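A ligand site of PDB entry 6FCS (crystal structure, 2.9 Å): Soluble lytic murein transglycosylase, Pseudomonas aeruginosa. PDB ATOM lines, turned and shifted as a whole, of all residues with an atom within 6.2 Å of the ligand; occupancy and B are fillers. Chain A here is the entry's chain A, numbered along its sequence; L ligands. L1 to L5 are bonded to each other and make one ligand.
O of Asp 480 sits at hydrogen-bond distance from N1 of LG2 L2, at 3.2 Å.
The backbone carbonyl oxygen (O) of Arg 482 lies within hydrogen-bond range of an oxygen (O4) of LG3 L3 (3.3 Å).
The guanidinium group (NE) of Arg 397 sits at hydrogen-bond distance from an oxygen (O5) of LG3 L3, 3.2 Å away.
The backbone NH of Gly 489 sits at hydrogen-bond distance from the backbone carbonyl oxygen of Ala 481 (3.2 Å).
The side-chain carboxylate of Asp 480 lies within salt-bridge range of the guanidinium group of Arg 397.
Merely in contact with the ligand: Ile 394 (3.6 Å), Tyr 401 (3.4 Å), Phe 426 (3.6 Å), Arg 430 (3.4 Å), Met 478 (3.3 Å), Ala 481 (3.9 Å), Thr 488 (3.97 Å), Gln 513 (3.8 Å) and Ile 516 (3.7 Å).
Hydrophobic or aromatic side chains within 4 Å of the ligand: Ile 394, Tyr 401, Phe 426, Met 478 and Ile 516.
Within 4 Å of the ligand: Ile 394, Arg 397, Tyr 401, Phe 426, Arg 430, Met 478, Asp 480, Ala 481, Arg 482, Thr 488, Gln 513 and Ile 516.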
ATOM      1  N   VAL A 393      -7.945  22.842 -30.829  1.00  0.00           N
ATOM      2  CA  VAL A 393      -6.830  21.986 -30.424  1.00  0.00           C
ATOM      3  C   VAL A 393      -7.063  21.523 -28.995  1.00  0.00           C
ATOM      4  O   VAL A 393      -6.941  20.335 -28.685  1.00  0.00           O
ATOM      5  CB  VAL A 393      -5.452  22.732 -30.458  1.00  0.00           C
ATOM      6  CG1 VAL A 393      -4.291  21.749 -30.271  1.00  0.00           C
ATOM      7  CG2 VAL A 393      -5.237  23.513 -31.758  1.00  0.00           C
ATOM      8  N   ILE A 394      -7.446  22.468 -28.143  1.00  0.00           N
ATOM      9  CA  ILE A 394      -7.396  22.319 -26.701  1.00  0.00           C
ATOM     10  C   ILE A 394      -8.544  21.460 -26.177  1.00  0.00           C
ATOM     11  O   ILE A 394      -8.356  20.663 -25.258  1.00  0.00           O
ATOM     12  CB  ILE A 394      -7.393  23.716 -26.025  1.00  0.00           C
ATOM     13  CG1 ILE A 394      -6.190  24.535 -26.529  1.00  0.00           C
ATOM     14  CG2 ILE A 394      -7.340  23.596 -24.504  1.00  0.00           C
ATOM     15  CD1 ILE A 394      -6.250  26.022 -26.221  1.00  0.00           C
ATOM     16  N   ARG A 397      -7.742  17.884 -27.276  1.00  0.00           N
ATOM     17  CA  ARG A 397      -6.658  17.403 -26.421  1.00  0.00           C
ATOM     18  C   ARG A 397      -7.191  16.961 -25.068  1.00  0.00           C
ATOM     19  O   ARG A 397      -6.843  15.864 -24.601  1.00  0.00           O
ATOM     20  CB  ARG A 397      -5.589  18.504 -26.261  1.00  0.00           C
ATOM     21  CG  ARG A 397      -4.163  17.979 -26.123  1.00  0.00           C
ATOM     22  CD  ARG A 397      -3.152  18.997 -26.616  1.00  0.00           C
ATOM     23  NE  ARG A 397      -3.203  20.246 -25.836  1.00  0.00           N
ATOM     24  CZ  ARG A 397      -2.783  21.443 -26.256  1.00  0.00           C
ATOM     25  NH1 ARG A 397      -2.271  21.630 -27.472  1.00  0.00           N
ATOM     26  NH2 ARG A 397      -2.896  22.488 -25.427  1.00  0.00           N
ATOM     27  N   ARG A 398      -8.042  17.793 -24.460  1.00  0.00           N
ATOM     28  CA  ARG A 398      -8.660  17.510 -23.152  1.00  0.00           C
ATOM     29  C   ARG A 398      -9.480  16.217 -23.153  1.00  0.00           C
ATOM     30  O   ARG A 398      -9.414  15.439 -22.192  1.00  0.00           O
ATOM     31  CB  ARG A 398      -9.551  18.684 -22.735  1.00  0.00           C
ATOM     32  CG  ARG A 398     -10.346  18.475 -21.448  1.00  0.00           C
ATOM     33  CD  ARG A 398     -11.369  19.577 -21.269  1.00  0.00           C
ATOM     34  NE  ARG A 398     -10.713  20.872 -21.108  1.00  0.00           N
ATOM     35  CZ  ARG A 398     -10.763  21.905 -21.954  1.00  0.00           C
ATOM     36  NH1 ARG A 398     -11.485  21.871 -23.074  1.00  0.00           N
ATOM     37  NH2 ARG A 398     -10.091  23.015 -21.652  1.00  0.00           N
ATOM     38  N   TYR A 401      -6.901  13.181 -23.072  1.00  0.00           N
ATOM     39  CA  TYR A 401      -6.270  12.928 -21.760  1.00  0.00           C
ATOM     40  C   TYR A 401      -7.228  12.223 -20.804  1.00  0.00           C
ATOM     41  O   TYR A 401      -6.904  11.192 -20.212  1.00  0.00           O
ATOM     42  CB  TYR A 401      -5.825  14.229 -21.082  1.00  0.00           C
ATOM     43  CG  TYR A 401      -4.802  15.110 -21.804  1.00  0.00           C
ATOM     44  CD1 TYR A 401      -4.090  14.665 -22.936  1.00  0.00           C
ATOM     45  CD2 TYR A 401      -4.523  16.386 -21.306  1.00  0.00           C
ATOM     46  CE1 TYR A 401      -3.159  15.489 -23.564  1.00  0.00           C
ATOM     47  CE2 TYR A 401      -3.590  17.211 -21.924  1.00  0.00           C
ATOM     48  CZ  TYR A 401      -2.914  16.760 -23.035  1.00  0.00           C
ATOM     49  OH  TYR A 401      -2.000  17.610 -23.619  1.00  0.00           O
ATOM     50  N   PHE A 426       2.100  15.085 -30.172  1.00  0.00           N
ATOM     51  CA  PHE A 426       2.208  15.117 -28.713  1.00  0.00           C
ATOM     52  C   PHE A 426       1.261  14.133 -27.991  1.00  0.00           C
ATOM     53  O   PHE A 426       1.713  13.403 -27.112  1.00  0.00           O
ATOM     54  CB  PHE A 426       2.059  16.536 -28.143  1.00  0.00           C
ATOM     55  CG  PHE A 426       1.961  16.571 -26.637  1.00  0.00           C
ATOM     56  CD1 PHE A 426       0.745  16.373 -25.986  1.00  0.00           C
ATOM     57  CD2 PHE A 426       3.105  16.742 -25.868  1.00  0.00           C
ATOM     58  CE1 PHE A 426       0.672  16.362 -24.608  1.00  0.00           C
ATOM     59  CE2 PHE A 426       3.026  16.752 -24.480  1.00  0.00           C
ATOM     60  CZ  PHE A 426       1.815  16.562 -23.852  1.00  0.00           C
ATOM     61  N   ARG A 430       2.245  11.093 -25.755  1.00  0.00           N
ATOM     62  CA  ARG A 430       1.721  11.074 -24.396  1.00  0.00           C
ATOM     63  C   ARG A 430       1.032   9.752 -24.097  1.00  0.00           C
ATOM     64  O   ARG A 430       1.308   9.123 -23.085  1.00  0.00           O
ATOM     65  CB  ARG A 430       0.760  12.241 -24.157  1.00  0.00           C
ATOM     66  CG  ARG A 430       0.384  12.462 -22.688  1.00  0.00           C
ATOM     67  CD  ARG A 430      -0.900  13.268 -22.520  1.00  0.00           C
ATOM     68  NE  ARG A 430      -1.904  12.526 -21.724  1.00  0.00           N
ATOM     69  CZ  ARG A 430      -2.374  12.852 -20.511  1.00  0.00           C
ATOM     70  NH1 ARG A 430      -1.962  13.949 -19.865  1.00  0.00           N
ATOM     71  NH2 ARG A 430      -3.284  12.071 -19.935  1.00  0.00           N
ATOM     72  N   MET A 478       4.411  19.718 -28.527  1.00  0.00           N
ATOM     73  CA  MET A 478       3.231  20.513 -28.167  1.00  0.00           C
ATOM     74  C   MET A 478       3.568  21.992 -28.344  1.00  0.00           C
ATOM     75  O   MET A 478       4.186  22.605 -27.474  1.00  0.00           O
ATOM     76  CB  MET A 478       2.805  20.229 -26.725  1.00  0.00           C
ATOM     77  CG  MET A 478       1.479  20.871 -26.329  1.00  0.00           C
ATOM     78  SD  MET A 478       0.829  20.223 -24.786  1.00  0.00           S
ATOM     79  CE  MET A 478       1.362  21.458 -23.614  1.00  0.00           C
ATOM     80  N   ASP A 480       2.057  24.809 -28.188  1.00  0.00           N
ATOM     81  CA  ASP A 480       1.550  25.821 -27.235  1.00  0.00           C
ATOM     82  C   ASP A 480       1.801  25.437 -25.762  1.00  0.00           C
ATOM     83  O   ASP A 480       0.975  25.705 -24.892  1.00  0.00           O
ATOM     84  CB  ASP A 480       0.063  26.150 -27.512  1.00  0.00           C
ATOM     85  CG  ASP A 480      -0.911  25.029 -27.123  1.00  0.00           C
ATOM     86  OD1 ASP A 480      -0.529  23.834 -27.156  1.00  0.00           O
ATOM     87  OD2 ASP A 480      -2.079  25.346 -26.800  1.00  0.00           O
ATOM     88  N   ALA A 481       2.965  24.835 -25.501  1.00  0.00           N
ATOM     89  CA  ALA A 481       3.329  24.414 -24.139  1.00  0.00           C
ATOM     90  C   ALA A 481       3.633  25.597 -23.221  1.00  0.00           C
ATOM     91  O   ALA A 481       3.869  26.714 -23.686  1.00  0.00           O
ATOM     92  CB  ALA A 481       4.503  23.445 -24.176  1.00  0.00           C
ATOM     93  N   ARG A 482       3.616  25.333 -21.926  1.00  0.00           N
ATOM     94  CA  ARG A 482       3.822  26.358 -20.912  1.00  0.00           C
ATOM     95  C   ARG A 482       4.223  25.711 -19.589  1.00  0.00           C
ATOM     96  O   ARG A 482       3.442  24.968 -19.001  1.00  0.00           O
ATOM     97  CB  ARG A 482       2.567  27.206 -20.725  1.00  0.00           C
ATOM     98  CG  ARG A 482       2.859  28.549 -20.081  1.00  0.00           C
ATOM     99  CD  ARG A 482       1.605  29.226 -19.543  1.00  0.00           C
ATOM    100  NE  ARG A 482       1.869  30.635 -19.211  1.00  0.00           N
ATOM    101  CZ  ARG A 482       2.485  31.072 -18.114  1.00  0.00           C
ATOM    102  NH1 ARG A 482       2.935  30.228 -17.180  1.00  0.00           N
ATOM    103  NH2 ARG A 482       2.659  32.376 -17.935  1.00  0.00           N
ATOM    104  N   SER A 483       5.441  26.017 -19.115  1.00  0.00           N
ATOM    105  CA  SER A 483       5.982  25.413 -17.898  1.00  0.00           C
ATOM    106  C   SER A 483       5.411  26.059 -16.639  1.00  0.00           C
ATOM    107  O   SER A 483       4.619  27.003 -16.716  1.00  0.00           O
ATOM    108  CB  SER A 483       7.518  25.515 -17.888  1.00  0.00           C
ATOM    109  OG  SER A 483       7.946  26.868 -17.816  1.00  0.00           O
ATOM    110  N   GLY A 484       5.808  25.545 -15.475  1.00  0.00           N
ATOM    111  CA  GLY A 484       5.452  26.138 -14.175  1.00  0.00           C
ATOM    112  C   GLY A 484       5.614  27.643 -14.086  1.00  0.00           C
ATOM    113  O   GLY A 484       4.752  28.330 -13.522  1.00  0.00           O
ATOM    114  N   THR A 488       7.823  28.980 -22.814  1.00  0.00           N
ATOM    115  CA  THR A 488       6.753  28.840 -23.816  1.00  0.00           C
ATOM    116  C   THR A 488       7.218  28.183 -25.118  1.00  0.00           C
ATOM    117  O   THR A 488       8.317  28.443 -25.607  1.00  0.00           O
ATOM    118  CB  THR A 488       6.142  30.224 -24.135  1.00  0.00           C
ATOM    119  OG1 THR A 488       6.099  31.035 -22.956  1.00  0.00           O
ATOM    120  CG2 THR A 488       4.728  30.083 -24.718  1.00  0.00           C
ATOM    121  N   GLY A 489       6.358  27.322 -25.674  1.00  0.00           N
ATOM    122  CA  GLY A 489       6.517  26.809 -27.032  1.00  0.00           C
ATOM    123  C   GLY A 489       7.429  25.600 -27.211  1.00  0.00           C
ATOM    124  O   GLY A 489       7.990  25.087 -26.249  1.00  0.00           O
ATOM    125  N   GLN A 492      10.606  25.747 -25.450  1.00  0.00           N
ATOM    126  CA  GLN A 492      10.417  26.310 -24.101  1.00  0.00           C
ATOM    127  C   GLN A 492      11.266  27.547 -23.789  1.00  0.00           C
ATOM    128  O   GLN A 492      12.090  27.565 -22.862  1.00  0.00           O
ATOM    129  CB  GLN A 492      10.590  25.206 -23.052  1.00  0.00           C
ATOM    130  CG  GLN A 492       9.491  24.149 -23.104  1.00  0.00           C
ATOM    131  CD  GLN A 492       8.183  24.605 -22.485  1.00  0.00           C
ATOM    132  OE1 GLN A 492       8.000  24.538 -21.269  1.00  0.00           O
ATOM    133  NE2 GLN A 492       7.258  25.064 -23.319  1.00  0.00           N
ATOM    134  N   GLN A 513       3.233  35.911 -26.051  1.00  0.00           N
ATOM    135  CA  GLN A 513       2.211  34.973 -26.534  1.00  0.00           C
ATOM    136  C   GLN A 513       2.437  34.486 -27.996  1.00  0.00           C
ATOM    137  O   GLN A 513       1.825  33.502 -28.411  1.00  0.00           O
ATOM    138  CB  GLN A 513       0.812  35.592 -26.366  1.00  0.00           C
ATOM    139  CG  GLN A 513      -0.296  34.626 -25.977  1.00  0.00           C
ATOM    140  CD  GLN A 513      -1.013  33.970 -27.158  1.00  0.00           C
ATOM    141  OE1 GLN A 513      -0.938  34.443 -28.293  1.00  0.00           O
ATOM    142  NE2 GLN A 513      -1.722  32.888 -26.878  1.00  0.00           N
ATOM    143  N   ILE A 516       3.956  30.613 -29.556  1.00  0.00           N
ATOM    144  CA  ILE A 516       3.177  29.433 -29.966  1.00  0.00           C
ATOM    145  C   ILE A 516       3.461  29.094 -31.439  1.00  0.00           C
ATOM    146  O   ILE A 516       3.441  27.915 -31.810  1.00  0.00           O
ATOM    147  CB  ILE A 516       1.650  29.639 -29.751  1.00  0.00           C
ATOM    148  CG1 ILE A 516       1.271  29.550 -28.258  1.00  0.00           C
ATOM    149  CG2 ILE A 516       0.835  28.576 -30.476  1.00  0.00           C
ATOM    150  CD1 ILE A 516       2.146  30.278 -27.274  1.00  0.00           C
HETATM  151  C1  LIG L   1      -6.735  31.530 -23.993  1.00  0.00           C
HETATM  152  C2  LIG L   1      -6.349  30.706 -22.721  1.00  0.00           C
HETATM  153  C3  LIG L   1      -4.961  30.031 -22.765  1.00  0.00           C
HETATM  154  C4  LIG L   1      -4.649  29.380 -24.140  1.00  0.00           C
HETATM  155  C5  LIG L   1      -4.640  30.496 -25.209  1.00  0.00           C
HETATM  156  C6  LIG L   1      -4.313  29.980 -26.634  1.00  0.00           C
HETATM  157  C7  LIG L   1      -5.681  32.617 -21.135  1.00  0.00           C
HETATM  158  C8  LIG L   1      -5.836  33.312 -19.767  1.00  0.00           C
HETATM  159  N1  LIG L   1      -6.507  31.395 -21.403  1.00  0.00           N
HETATM  160  O1  LIG L   1      -8.158  31.363 -24.185  1.00  0.00           O
HETATM  161  O2  LIG L   1      -4.980  29.052 -21.728  1.00  0.00           O
HETATM  162  O3  LIG L   1      -3.363  28.717 -24.105  1.00  0.00           O
HETATM  163  O4  LIG L   1      -5.910  31.218 -25.161  1.00  0.00           O
HETATM  164  O5  LIG L   1      -3.056  29.301 -26.662  1.00  0.00           O
HETATM  165  O6  LIG L   1      -4.912  33.095 -21.932  1.00  0.00           O
HETATM  166  C9  LIG L   1      -8.673  31.551 -25.511  1.00  0.00           C
HETATM  167  C1  LG2 L   2      -3.314  27.359 -23.642  1.00  0.00           C
HETATM  168  C2  LG2 L   2      -2.083  27.267 -22.681  1.00  0.00           C
HETATM  169  C3  LG2 L   2      -1.886  25.757 -22.442  1.00  0.00           C
HETATM  170  C4  LG2 L   2      -3.146  25.111 -21.845  1.00  0.00           C
HETATM  171  C5  LG2 L   2      -4.438  25.490 -22.600  1.00  0.00           C
HETATM  172  C6  LG2 L   2      -5.691  25.234 -21.765  1.00  0.00           C
HETATM  173  C7  LG2 L   2      -0.279  28.910 -23.116  1.00  0.00           C
HETATM  174  C8  LG2 L   2       0.942  29.210 -23.926  1.00  0.00           C
HETATM  175  N1  LG2 L   2      -0.886  27.744 -23.357  1.00  0.00           N
HETATM  176  O1  LG2 L   2      -0.790  25.661 -21.558  1.00  0.00           O
HETATM  177  O2  LG2 L   2      -3.063  23.684 -21.969  1.00  0.00           O
HETATM  178  O3  LG2 L   2      -4.421  26.924 -22.912  1.00  0.00           O
HETATM  179  O4  LG2 L   2      -5.731  25.998 -20.561  1.00  0.00           O
HETATM  180  O5  LG2 L   2      -0.674  29.734 -22.279  1.00  0.00           O
HETATM  181  C1  LG3 L   3      -2.348  22.889 -21.062  1.00  0.00           C
HETATM  182  C2  LG3 L   3      -2.636  21.394 -21.002  1.00  0.00           C
HETATM  183  C3  LG3 L   3      -1.776  20.833 -19.847  1.00  0.00           C
HETATM  184  C4  LG3 L   3      -0.279  21.246 -19.859  1.00  0.00           C
HETATM  185  C5  LG3 L   3      -0.139  22.736 -20.346  1.00  0.00           C
HETATM  186  C6  LG3 L   3       1.231  23.217 -20.768  1.00  0.00           C
HETATM  187  C7  LG3 L   3      -4.975  20.875 -21.809  1.00  0.00           C
HETATM  188  C8  LG3 L   3      -6.417  20.812 -21.369  1.00  0.00           C
HETATM  189  C9  LG3 L   3      -2.188  18.725 -18.499  1.00  0.00           C
HETATM  190  C10 LG3 L   3      -3.453  18.990 -17.600  1.00  0.00           C
HETATM  191  C11 LG3 L   3      -2.101  17.221 -18.855  1.00  0.00           C
HETATM  192  O1  LG3 L   3      -2.046  19.400 -19.778  1.00  0.00           O
HETATM  193  O2  LG3 L   3       0.307  21.275 -18.554  1.00  0.00           O
HETATM  194  O3  LG3 L   3      -0.959  22.958 -21.466  1.00  0.00           O
HETATM  195  O4  LG3 L   3       2.289  22.296 -20.591  1.00  0.00           O
HETATM  196  O5  LG3 L   3      -4.676  20.572 -22.966  1.00  0.00           O
HETATM  197  O6  LG3 L   3      -3.880  18.098 -16.897  1.00  0.00           O
HETATM  198  N1  LG3 L   3      -4.092  21.247 -20.863  1.00  0.00           N
HETATM  199  C1  LG4 L   4       1.120  20.446 -17.733  1.00  0.00           C
HETATM  200  C2  LG4 L   4       2.389  19.866 -18.391  1.00  0.00           C
HETATM  201  C3  LG4 L   4       3.422  19.417 -17.348  1.00  0.00           C
HETATM  202  C4  LG4 L   4       3.534  20.274 -16.071  1.00  0.00           C
HETATM  203  C5  LG4 L   4       2.162  20.798 -15.588  1.00  0.00           C
HETATM  204  C6  LG4 L   4       2.325  21.872 -14.515  1.00  0.00           C
HETATM  205  C7  LG4 L   4       1.474  17.621 -19.089  1.00  0.00           C
HETATM  206  C8  LG4 L   4       1.244  16.709 -20.255  1.00  0.00           C
HETATM  207  N1  LG4 L   4       2.049  18.800 -19.353  1.00  0.00           N
HETATM  208  O1  LG4 L   4       4.702  19.334 -17.967  1.00  0.00           O
HETATM  209  O2  LG4 L   4       4.147  19.496 -15.044  1.00  0.00           O
HETATM  210  O3  LG4 L   4       1.506  21.388 -16.688  1.00  0.00           O
HETATM  211  O4  LG4 L   4       1.536  21.638 -13.352  1.00  0.00           O
HETATM  212  O5  LG4 L   4       1.130  17.236 -17.972  1.00  0.00           O
HETATM  213  O1  LG5 L   5      -5.592  22.556 -17.943  1.00  0.00           O
HETATM  214  N1  LG5 L   5      -4.146  20.292 -17.513  1.00  0.00           N
HETATM  215  C1  LG5 L   5      -5.318  20.530 -16.648  1.00  0.00           C
HETATM  216  C2  LG5 L   5      -4.839  20.681 -15.190  1.00  0.00           C
HETATM  217  C3  LG5 L   5      -6.069  21.810 -17.116  1.00  0.00           C
HETATM  218  N2  LG5 L   5      -7.383  22.128 -16.564  1.00  0.00           N
